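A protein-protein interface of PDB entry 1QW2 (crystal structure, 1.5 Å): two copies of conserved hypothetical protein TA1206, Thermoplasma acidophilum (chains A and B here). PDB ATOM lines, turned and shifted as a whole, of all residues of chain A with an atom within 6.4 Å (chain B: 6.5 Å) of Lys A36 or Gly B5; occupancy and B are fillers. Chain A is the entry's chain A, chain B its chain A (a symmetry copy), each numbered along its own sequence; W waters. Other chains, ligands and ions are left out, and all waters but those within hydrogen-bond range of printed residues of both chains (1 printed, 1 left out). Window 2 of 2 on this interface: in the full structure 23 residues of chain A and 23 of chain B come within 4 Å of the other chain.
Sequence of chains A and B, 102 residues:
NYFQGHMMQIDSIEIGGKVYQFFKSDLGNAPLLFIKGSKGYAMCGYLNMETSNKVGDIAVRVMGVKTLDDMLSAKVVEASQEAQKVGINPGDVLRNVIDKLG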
ATOM      1  N   VAL A  19      27.616   7.749 -21.464  1.00  0.00           N
ATOM      2  CA  VAL A  19      27.763   7.269 -20.095  1.00  0.00           C
ATOM      3  C   VAL A  19      27.929   5.755 -20.042  1.00  0.00           C
ATOM      4  O   VAL A  19      27.230   5.014 -20.736  1.00  0.00           O
ATOM      5  CB  VAL A  19      26.545   7.665 -19.235  1.00  0.00           C
ATOM      6  CG1 VAL A  19      26.792   7.293 -17.780  1.00  0.00           C
ATOM      7  CG2 VAL A  19      26.279   9.157 -19.368  1.00  0.00           C
ATOM      8  N   TYR A  20      28.859   5.303 -19.207  1.00  0.00           N
ATOM      9  CA  TYR A  20      29.140   3.881 -19.051  1.00  0.00           C
ATOM     10  C   TYR A  20      29.245   3.541 -17.575  1.00  0.00           C
ATOM     11  O   TYR A  20      29.575   4.394 -16.750  1.00  0.00           O
ATOM     12  CB  TYR A  20      30.467   3.523 -19.727  1.00  0.00           C
ATOM     13  CG  TYR A  20      30.506   3.798 -21.208  1.00  0.00           C
ATOM     14  CD1 TYR A  20      30.144   2.819 -22.129  1.00  0.00           C
ATOM     15  CD2 TYR A  20      30.885   5.049 -21.689  1.00  0.00           C
ATOM     16  CE1 TYR A  20      30.158   3.081 -23.500  1.00  0.00           C
ATOM     17  CE2 TYR A  20      30.901   5.323 -23.050  1.00  0.00           C
ATOM     18  CZ  TYR A  20      30.536   4.336 -23.950  1.00  0.00           C
ATOM     19  OH  TYR A  20      30.557   4.616 -25.296  1.00  0.00           O
ATOM     20  N   GLN A  21      28.967   2.287 -17.243  1.00  0.00           N
ATOM     21  CA  GLN A  21      29.068   1.839 -15.867  1.00  0.00           C
ATOM     22  C   GLN A  21      30.278   0.923 -15.748  1.00  0.00           C
ATOM     23  O   GLN A  21      30.364  -0.090 -16.445  1.00  0.00           O
ATOM     24  CB  GLN A  21      27.805   1.080 -15.455  1.00  0.00           C
ATOM     25  CG  GLN A  21      26.533   1.910 -15.541  1.00  0.00           C
ATOM     26  CD  GLN A  21      26.529   3.087 -14.582  1.00  0.00           C
ATOM     27  OE1 GLN A  21      25.662   3.957 -14.657  1.00  0.00           O
ATOM     28  NE2 GLN A  21      27.495   3.116 -13.671  1.00  0.00           N
ATOM     29  N   PHE A  22      31.229   1.301 -14.901  1.00  0.00           N
ATOM     30  CA  PHE A  22      32.409   0.482 -14.673  1.00  0.00           C
ATOM     31  C   PHE A  22      32.206  -0.232 -13.348  1.00  0.00           C
ATOM     32  O   PHE A  22      31.845   0.388 -12.346  1.00  0.00           O
ATOM     33  CB  PHE A  22      33.683   1.325 -14.587  1.00  0.00           C
ATOM     34  CG  PHE A  22      34.890   0.542 -14.144  1.00  0.00           C
ATOM     35  CD1 PHE A  22      35.459  -0.418 -14.978  1.00  0.00           C
ATOM     36  CD2 PHE A  22      35.434   0.732 -12.878  1.00  0.00           C
ATOM     37  CE1 PHE A  22      36.550  -1.179 -14.562  1.00  0.00           C
ATOM     38  CE2 PHE A  22      36.527  -0.024 -12.451  1.00  0.00           C
ATOM     39  CZ  PHE A  22      37.085  -0.981 -13.293  1.00  0.00           C
ATOM     40  N   PHE A  23      32.433  -1.537 -13.347  1.00  0.00           N
ATOM     41  CA  PHE A  23      32.278  -2.330 -12.142  1.00  0.00           C
ATOM     42  C   PHE A  23      33.501  -3.204 -11.926  1.00  0.00           C
ATOM     43  O   PHE A  23      34.057  -3.751 -12.875  1.00  0.00           O
ATOM     44  CB  PHE A  23      31.025  -3.211 -12.248  1.00  0.00           C
ATOM     45  CG  PHE A  23      30.847  -4.165 -11.098  1.00  0.00           C
ATOM     46  CD1 PHE A  23      31.339  -5.470 -11.170  1.00  0.00           C
ATOM     47  CD2 PHE A  23      30.190  -3.760  -9.942  1.00  0.00           C
ATOM     48  CE1 PHE A  23      31.172  -6.355 -10.100  1.00  0.00           C
ATOM     49  CE2 PHE A  23      30.020  -4.633  -8.874  1.00  0.00           C
ATOM     50  CZ  PHE A  23      30.512  -5.935  -8.953  1.00  0.00           C
ATOM     51  N   PHE A  34      34.048  -5.108 -15.520  1.00  0.00           N
ATOM     52  CA  PHE A  34      33.414  -4.872 -16.801  1.00  0.00           C
ATOM     53  C   PHE A  34      33.039  -3.409 -16.956  1.00  0.00           C
ATOM     54  O   PHE A  34      33.026  -2.648 -15.984  1.00  0.00           O
ATOM     55  CB  PHE A  34      32.165  -5.773 -16.967  1.00  0.00           C
ATOM     56  CG  PHE A  34      31.018  -5.449 -16.033  1.00  0.00           C
ATOM     57  CD1 PHE A  34      30.208  -4.332 -16.248  1.00  0.00           C
ATOM     58  CD2 PHE A  34      30.714  -6.294 -14.973  1.00  0.00           C
ATOM     59  CE1 PHE A  34      29.111  -4.066 -15.420  1.00  0.00           C
ATOM     60  CE2 PHE A  34      29.617  -6.036 -14.138  1.00  0.00           C
ATOM     61  CZ  PHE A  34      28.817  -4.924 -14.364  1.00  0.00           C
ATOM     62  N   ILE A  35      32.793  -3.017 -18.200  1.00  0.00           N
ATOM     63  CA  ILE A  35      32.363  -1.671 -18.543  1.00  0.00           C
ATOM     64  C   ILE A  35      31.113  -1.902 -19.378  1.00  0.00           C
ATOM     65  O   ILE A  35      31.160  -2.600 -20.392  1.00  0.00           O
ATOM     66  CB  ILE A  35      33.394  -0.919 -19.398  1.00  0.00           C
ATOM     67  CG1 ILE A  35      34.702  -0.762 -18.626  1.00  0.00           C
ATOM     68  CG2 ILE A  35      32.835   0.455 -19.785  1.00  0.00           C
ATOM     69  CD1 ILE A  35      35.813  -0.115 -19.433  1.00  0.00           C
ATOM     70  N   LYS A  36      29.997  -1.327 -18.956  1.00  0.00           N
ATOM     71  CA  LYS A  36      28.753  -1.524 -19.682  1.00  0.00           C
ATOM     72  C   LYS A  36      28.128  -0.241 -20.198  1.00  0.00           C
ATOM     73  O   LYS A  36      28.025   0.751 -19.477  1.00  0.00           O
ATOM     74  CB  LYS A  36      27.760  -2.277 -18.792  1.00  0.00           C
ATOM     75  CG  LYS A  36      26.427  -2.607 -19.455  1.00  0.00           C
ATOM     76  CD  LYS A  36      25.362  -1.581 -19.096  1.00  0.00           C
ATOM     77  CE  LYS A  36      24.023  -1.938 -19.729  1.00  0.00           C
ATOM     78  NZ  LYS A  36      22.906  -1.126 -19.166  1.00  0.00           N
ATOM     79  N   GLY A  37      27.725  -0.276 -21.464  1.00  0.00           N
ATOM     80  CA  GLY A  37      27.081   0.861 -22.089  1.00  0.00           C
ATOM     81  C   GLY A  37      25.649   0.467 -22.382  1.00  0.00           C
ATOM     82  O   GLY A  37      25.236  -0.643 -22.055  1.00  0.00           O
ATOM     83  N   SER A  38      24.886   1.358 -23.005  1.00  0.00           N
ATOM     84  CA  SER A  38      23.493   1.061 -23.309  1.00  0.00           C
ATOM     85  C   SER A  38      23.305   0.007 -24.399  1.00  0.00           C
ATOM     86  O   SER A  38      22.260  -0.636 -24.465  1.00  0.00           O
ATOM     87  CB  SER A  38      22.754   2.345 -23.710  1.00  0.00           C
ATOM     88  OG  SER A  38      23.301   2.910 -24.889  1.00  0.00           O
ATOM     89  N   LYS A  39      24.320  -0.185 -25.238  1.00  0.00           N
ATOM     90  CA  LYS A  39      24.225  -1.147 -26.334  1.00  0.00           C
ATOM     91  C   LYS A  39      25.012  -2.442 -26.141  1.00  0.00           C
ATOM     92  O   LYS A  39      24.648  -3.481 -26.691  1.00  0.00           O
ATOM     93  CB  LYS A  39      24.675  -0.486 -27.639  1.00  0.00           C
ATOM     94  CG  LYS A  39      23.892   0.763 -28.004  1.00  0.00           C
ATOM     95  CD  LYS A  39      24.407   1.368 -29.296  1.00  0.00           C
ATOM     96  CE  LYS A  39      23.700   2.675 -29.615  1.00  0.00           C
ATOM     97  NZ  LYS A  39      24.180   3.266 -30.895  1.00  0.00           N
ATOM     98  N   GLY A  40      26.096  -2.380 -25.376  1.00  0.00           N
ATOM     99  CA  GLY A  40      26.901  -3.570 -25.166  1.00  0.00           C
ATOM    100  C   GLY A  40      27.851  -3.417 -23.996  1.00  0.00           C
ATOM    101  O   GLY A  40      27.795  -2.430 -23.265  1.00  0.00           O
ATOM    102  N   TYR A  41      28.741  -4.388 -23.828  1.00  0.00           N
ATOM    103  CA  TYR A  41      29.678  -4.352 -22.719  1.00  0.00           C
ATOM    104  C   TYR A  41      31.025  -4.983 -23.044  1.00  0.00           C
ATOM    105  O   TYR A  41      31.174  -5.709 -24.034  1.00  0.00           O
ATOM    106  CB  TYR A  41      29.053  -5.077 -21.518  1.00  0.00           C
ATOM    107  CG  TYR A  41      28.698  -6.520 -21.820  1.00  0.00           C
ATOM    108  CD1 TYR A  41      29.638  -7.541 -21.668  1.00  0.00           C
ATOM    109  CD2 TYR A  41      27.437  -6.857 -22.316  1.00  0.00           C
ATOM    110  CE1 TYR A  41      29.329  -8.862 -22.008  1.00  0.00           C
ATOM    111  CE2 TYR A  41      27.121  -8.173 -22.657  1.00  0.00           C
ATOM    112  CZ  TYR A  41      28.071  -9.168 -22.502  1.00  0.00           C
ATOM    113  OH  TYR A  41      27.769 -10.464 -22.837  1.00  0.00           O
ATOM    114  N   ALA A  42      32.009  -4.668 -22.207  1.00  0.00           N
ATOM    115  CA  ALA A  42      33.355  -5.220 -22.315  1.00  0.00           C
ATOM    116  C   ALA A  42      33.609  -5.847 -20.953  1.00  0.00           C
ATOM    117  O   ALA A  42      33.276  -5.258 -19.927  1.00  0.00           O
ATOM    118  CB  ALA A  42      34.371  -4.120 -22.574  1.00  0.00           C
ATOM    119  N   LEU A 101      29.656   0.688 -27.858  1.00  0.00           N
ATOM    120  CA  LEU A 101      29.006  -0.058 -26.784  1.00  0.00           C
ATOM    121  C   LEU A 101      28.000   0.823 -26.051  1.00  0.00           C
ATOM    122  O   LEU A 101      27.248   0.348 -25.199  1.00  0.00           O
ATOM    123  CB  LEU A 101      30.046  -0.579 -25.788  1.00  0.00           C
ATOM    124  CG  LEU A 101      31.144  -1.482 -26.355  1.00  0.00           C
ATOM    125  CD1 LEU A 101      32.017  -1.996 -25.216  1.00  0.00           C
ATOM    126  CD2 LEU A 101      30.514  -2.646 -27.104  1.00  0.00           C
ATOM    127  N   PHE B   3      13.371   6.434 -17.043  1.00  0.00           N
ATOM    128  CA  PHE B   3      13.892   5.269 -17.744  1.00  0.00           C
ATOM    129  C   PHE B   3      15.029   4.650 -16.939  1.00  0.00           C
ATOM    130  O   PHE B   3      15.947   5.352 -16.516  1.00  0.00           O
ATOM    131  CB  PHE B   3      14.409   5.675 -19.127  1.00  0.00           C
ATOM    132  CG  PHE B   3      15.068   4.554 -19.882  1.00  0.00           C
ATOM    133  CD1 PHE B   3      14.325   3.462 -20.323  1.00  0.00           C
ATOM    134  CD2 PHE B   3      16.433   4.588 -20.150  1.00  0.00           C
ATOM    135  CE1 PHE B   3      14.933   2.419 -21.019  1.00  0.00           C
ATOM    136  CE2 PHE B   3      17.051   3.550 -20.845  1.00  0.00           C
ATOM    137  CZ  PHE B   3      16.299   2.464 -21.280  1.00  0.00           C
ATOM    138  N   GLN B   4      14.967   3.340 -16.723  1.00  0.00           N
ATOM    139  CA  GLN B   4      16.015   2.652 -15.975  1.00  0.00           C
ATOM    140  C   GLN B   4      17.070   2.139 -16.947  1.00  0.00           C
ATOM    141  O   GLN B   4      16.863   1.133 -17.629  1.00  0.00           O
ATOM    142  CB  GLN B   4      15.437   1.476 -15.181  1.00  0.00           C
ATOM    143  CG  GLN B   4      16.455   0.807 -14.265  1.00  0.00           C
ATOM    144  CD  GLN B   4      15.920  -0.445 -13.592  1.00  0.00           C
ATOM    145  OE1 GLN B   4      15.634  -1.445 -14.249  1.00  0.00           O
ATOM    146  NE2 GLN B   4      15.781  -0.392 -12.273  1.00  0.00           N
ATOM    147  N   GLY B   5      18.201   2.836 -17.009  1.00  0.00           N
ATOM    148  CA  GLY B   5      19.268   2.440 -17.910  1.00  0.00           C
ATOM    149  C   GLY B   5      20.086   1.266 -17.410  1.00  0.00           C
ATOM    150  O   GLY B   5      20.534   0.430 -18.196  1.00  0.00           O
ATOM    151  N   HIS B   6      20.289   1.204 -16.098  1.00  0.00           N
ATOM    152  CA  HIS B   6      21.058   0.122 -15.502  1.00  0.00           C
ATOM    153  C   HIS B   6      20.580  -0.160 -14.083  1.00  0.00           C
ATOM    154  O   HIS B   6      20.225   0.759 -13.347  1.00  0.00           O
ATOM    155  CB  HIS B   6      22.542   0.486 -15.466  1.00  0.00           C
ATOM    156  CG  HIS B   6      23.416  -0.618 -14.964  1.00  0.00           C
ATOM    157  ND1 HIS B   6      23.667  -1.757 -15.697  1.00  0.00           N
ATOM    158  CD2 HIS B   6      24.058  -0.781 -13.783  1.00  0.00           C
ATOM    159  CE1 HIS B   6      24.424  -2.576 -14.990  1.00  0.00           C
ATOM    160  NE2 HIS B   6      24.675  -2.008 -13.824  1.00  0.00           N
ATOM    161  N   MET B   7      20.570  -1.434 -13.704  1.00  0.00           N
ATOM    162  CA  MET B   7      20.144  -1.824 -12.367  1.00  0.00           C
ATOM    163  C   MET B   7      21.154  -2.777 -11.757  1.00  0.00           C
ATOM    164  O   MET B   7      21.707  -3.635 -12.443  1.00  0.00           O
ATOM    165  CB  MET B   7      18.765  -2.505 -12.396  1.00  0.00           C
ATOM    166  CG  MET B   7      18.748  -3.969 -12.863  1.00  0.00           C
ATOM    167  SD  MET B   7      19.448  -5.186 -11.694  1.00  0.00           S
ATOM    168  CE  MET B   7      18.182  -5.202 -10.422  1.00  0.00           C
ATOM    169  N   ASP B  26      22.405  -5.748 -14.635  1.00  0.00           N
ATOM    170  CA  ASP B  26      22.041  -5.919 -16.026  1.00  0.00           C
ATOM    171  C   ASP B  26      23.417  -6.030 -16.669  1.00  0.00           C
ATOM    172  O   ASP B  26      24.400  -5.511 -16.134  1.00  0.00           O
ATOM    173  CB  ASP B  26      21.332  -4.680 -16.587  1.00  0.00           C
ATOM    174  CG  ASP B  26      19.989  -4.427 -15.945  1.00  0.00           C
ATOM    175  OD1 ASP B  26      19.188  -5.378 -15.848  1.00  0.00           O
ATOM    176  OD2 ASP B  26      19.729  -3.269 -15.554  1.00  0.00           O
ATOM    177  N   LEU B  27      23.506  -6.725 -17.789  1.00  0.00           N
ATOM    178  CA  LEU B  27      24.774  -6.828 -18.490  1.00  0.00           C
ATOM    179  C   LEU B  27      24.440  -6.820 -19.970  1.00  0.00           C
ATOM    180  O   LEU B  27      24.702  -5.843 -20.667  1.00  0.00           O
ATOM    181  CB  LEU B  27      25.526  -8.110 -18.113  1.00  0.00           C
ATOM    182  CG  LEU B  27      26.923  -8.200 -18.742  1.00  0.00           C
ATOM    183  CD1 LEU B  27      27.806  -7.096 -18.170  1.00  0.00           C
ATOM    184  CD2 LEU B  27      27.538  -9.567 -18.466  1.00  0.00           C
ATOM    185  N   GLY B  28      23.836  -7.905 -20.440  1.00  0.00           N
ATOM    186  CA  GLY B  28      23.463  -7.989 -21.841  1.00  0.00           C
ATOM    187  C   GLY B  28      22.004  -8.376 -21.954  1.00  0.00           C
ATOM    188  O   GLY B  28      21.159  -7.837 -21.234  1.00  0.00           O
HETATM  189  O   HOH W   1      24.588  -3.923 -22.686  1.00  0.00           O
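Hydrophobic or aromatic side chains of chain B within 4 Å of the printed part of chain A: His B6 and Leu B27. Hydrophobic or aromatic side chains of chain A that line the printed part of chain B: Tyr A41. Among the printed residues, 5 pairs touch across the chains. Among the printed residues, no Asp or Glu carboxylate lies within 4 Å of a Lys or Arg side-chain nitrogen of the other chain.
O of Gln A21 lies within hydrogen-bond range of N of Lys A36, 2.8 Å away.
The side-chain amino group of Lys A36 sits at hydrogen-bond distance from the backbone carbonyl oxygen of Gly B5, at 3.0 Å.
Water W1 lies within hydrogen-bond range of the backbone carbonyl oxygen (O) of Leu B27 (2.8 Å), the backbone carbonyl oxygen (O) of Gly A37 (3.4 Å) and the backbone NH (N) of Gly A40 (3.4 Å).
NZ of Lys A36 touches ND1 of His B6, at 3.6 Å. Lys A36 touches Leu B27. CD2 of Tyr A41 touches O of Leu B27 (3.4 Å). Gly B28 touches Tyr A41 (CA to CE2, 3.8 Å).
Of chain B, only Gly B5, His B6 and Leu B27 come within 4 Å of Lys A36. Gly A37 touches none of the printed residues of chain B. Gly A40 touches none of the printed residues of chain B. Printed residues of chain B within 4 Å of Tyr A41: Leu B27 (3.4 Å) and Gly B28 (3.8 Å). Gly B5 touches just one residue of chain A: Lys A36 (3.0 Å). Of the printed residues of chain A, His B6 touches Lys A36 (3.6 Å). Printed residues of chain A within 4 Å of Leu B27: Lys A36 (3.9 Å) and Tyr A41 (3.4 Å). Printed residues of chain A within 4 Å of Gly B28: Tyr A41.
No position is printed for both chains.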
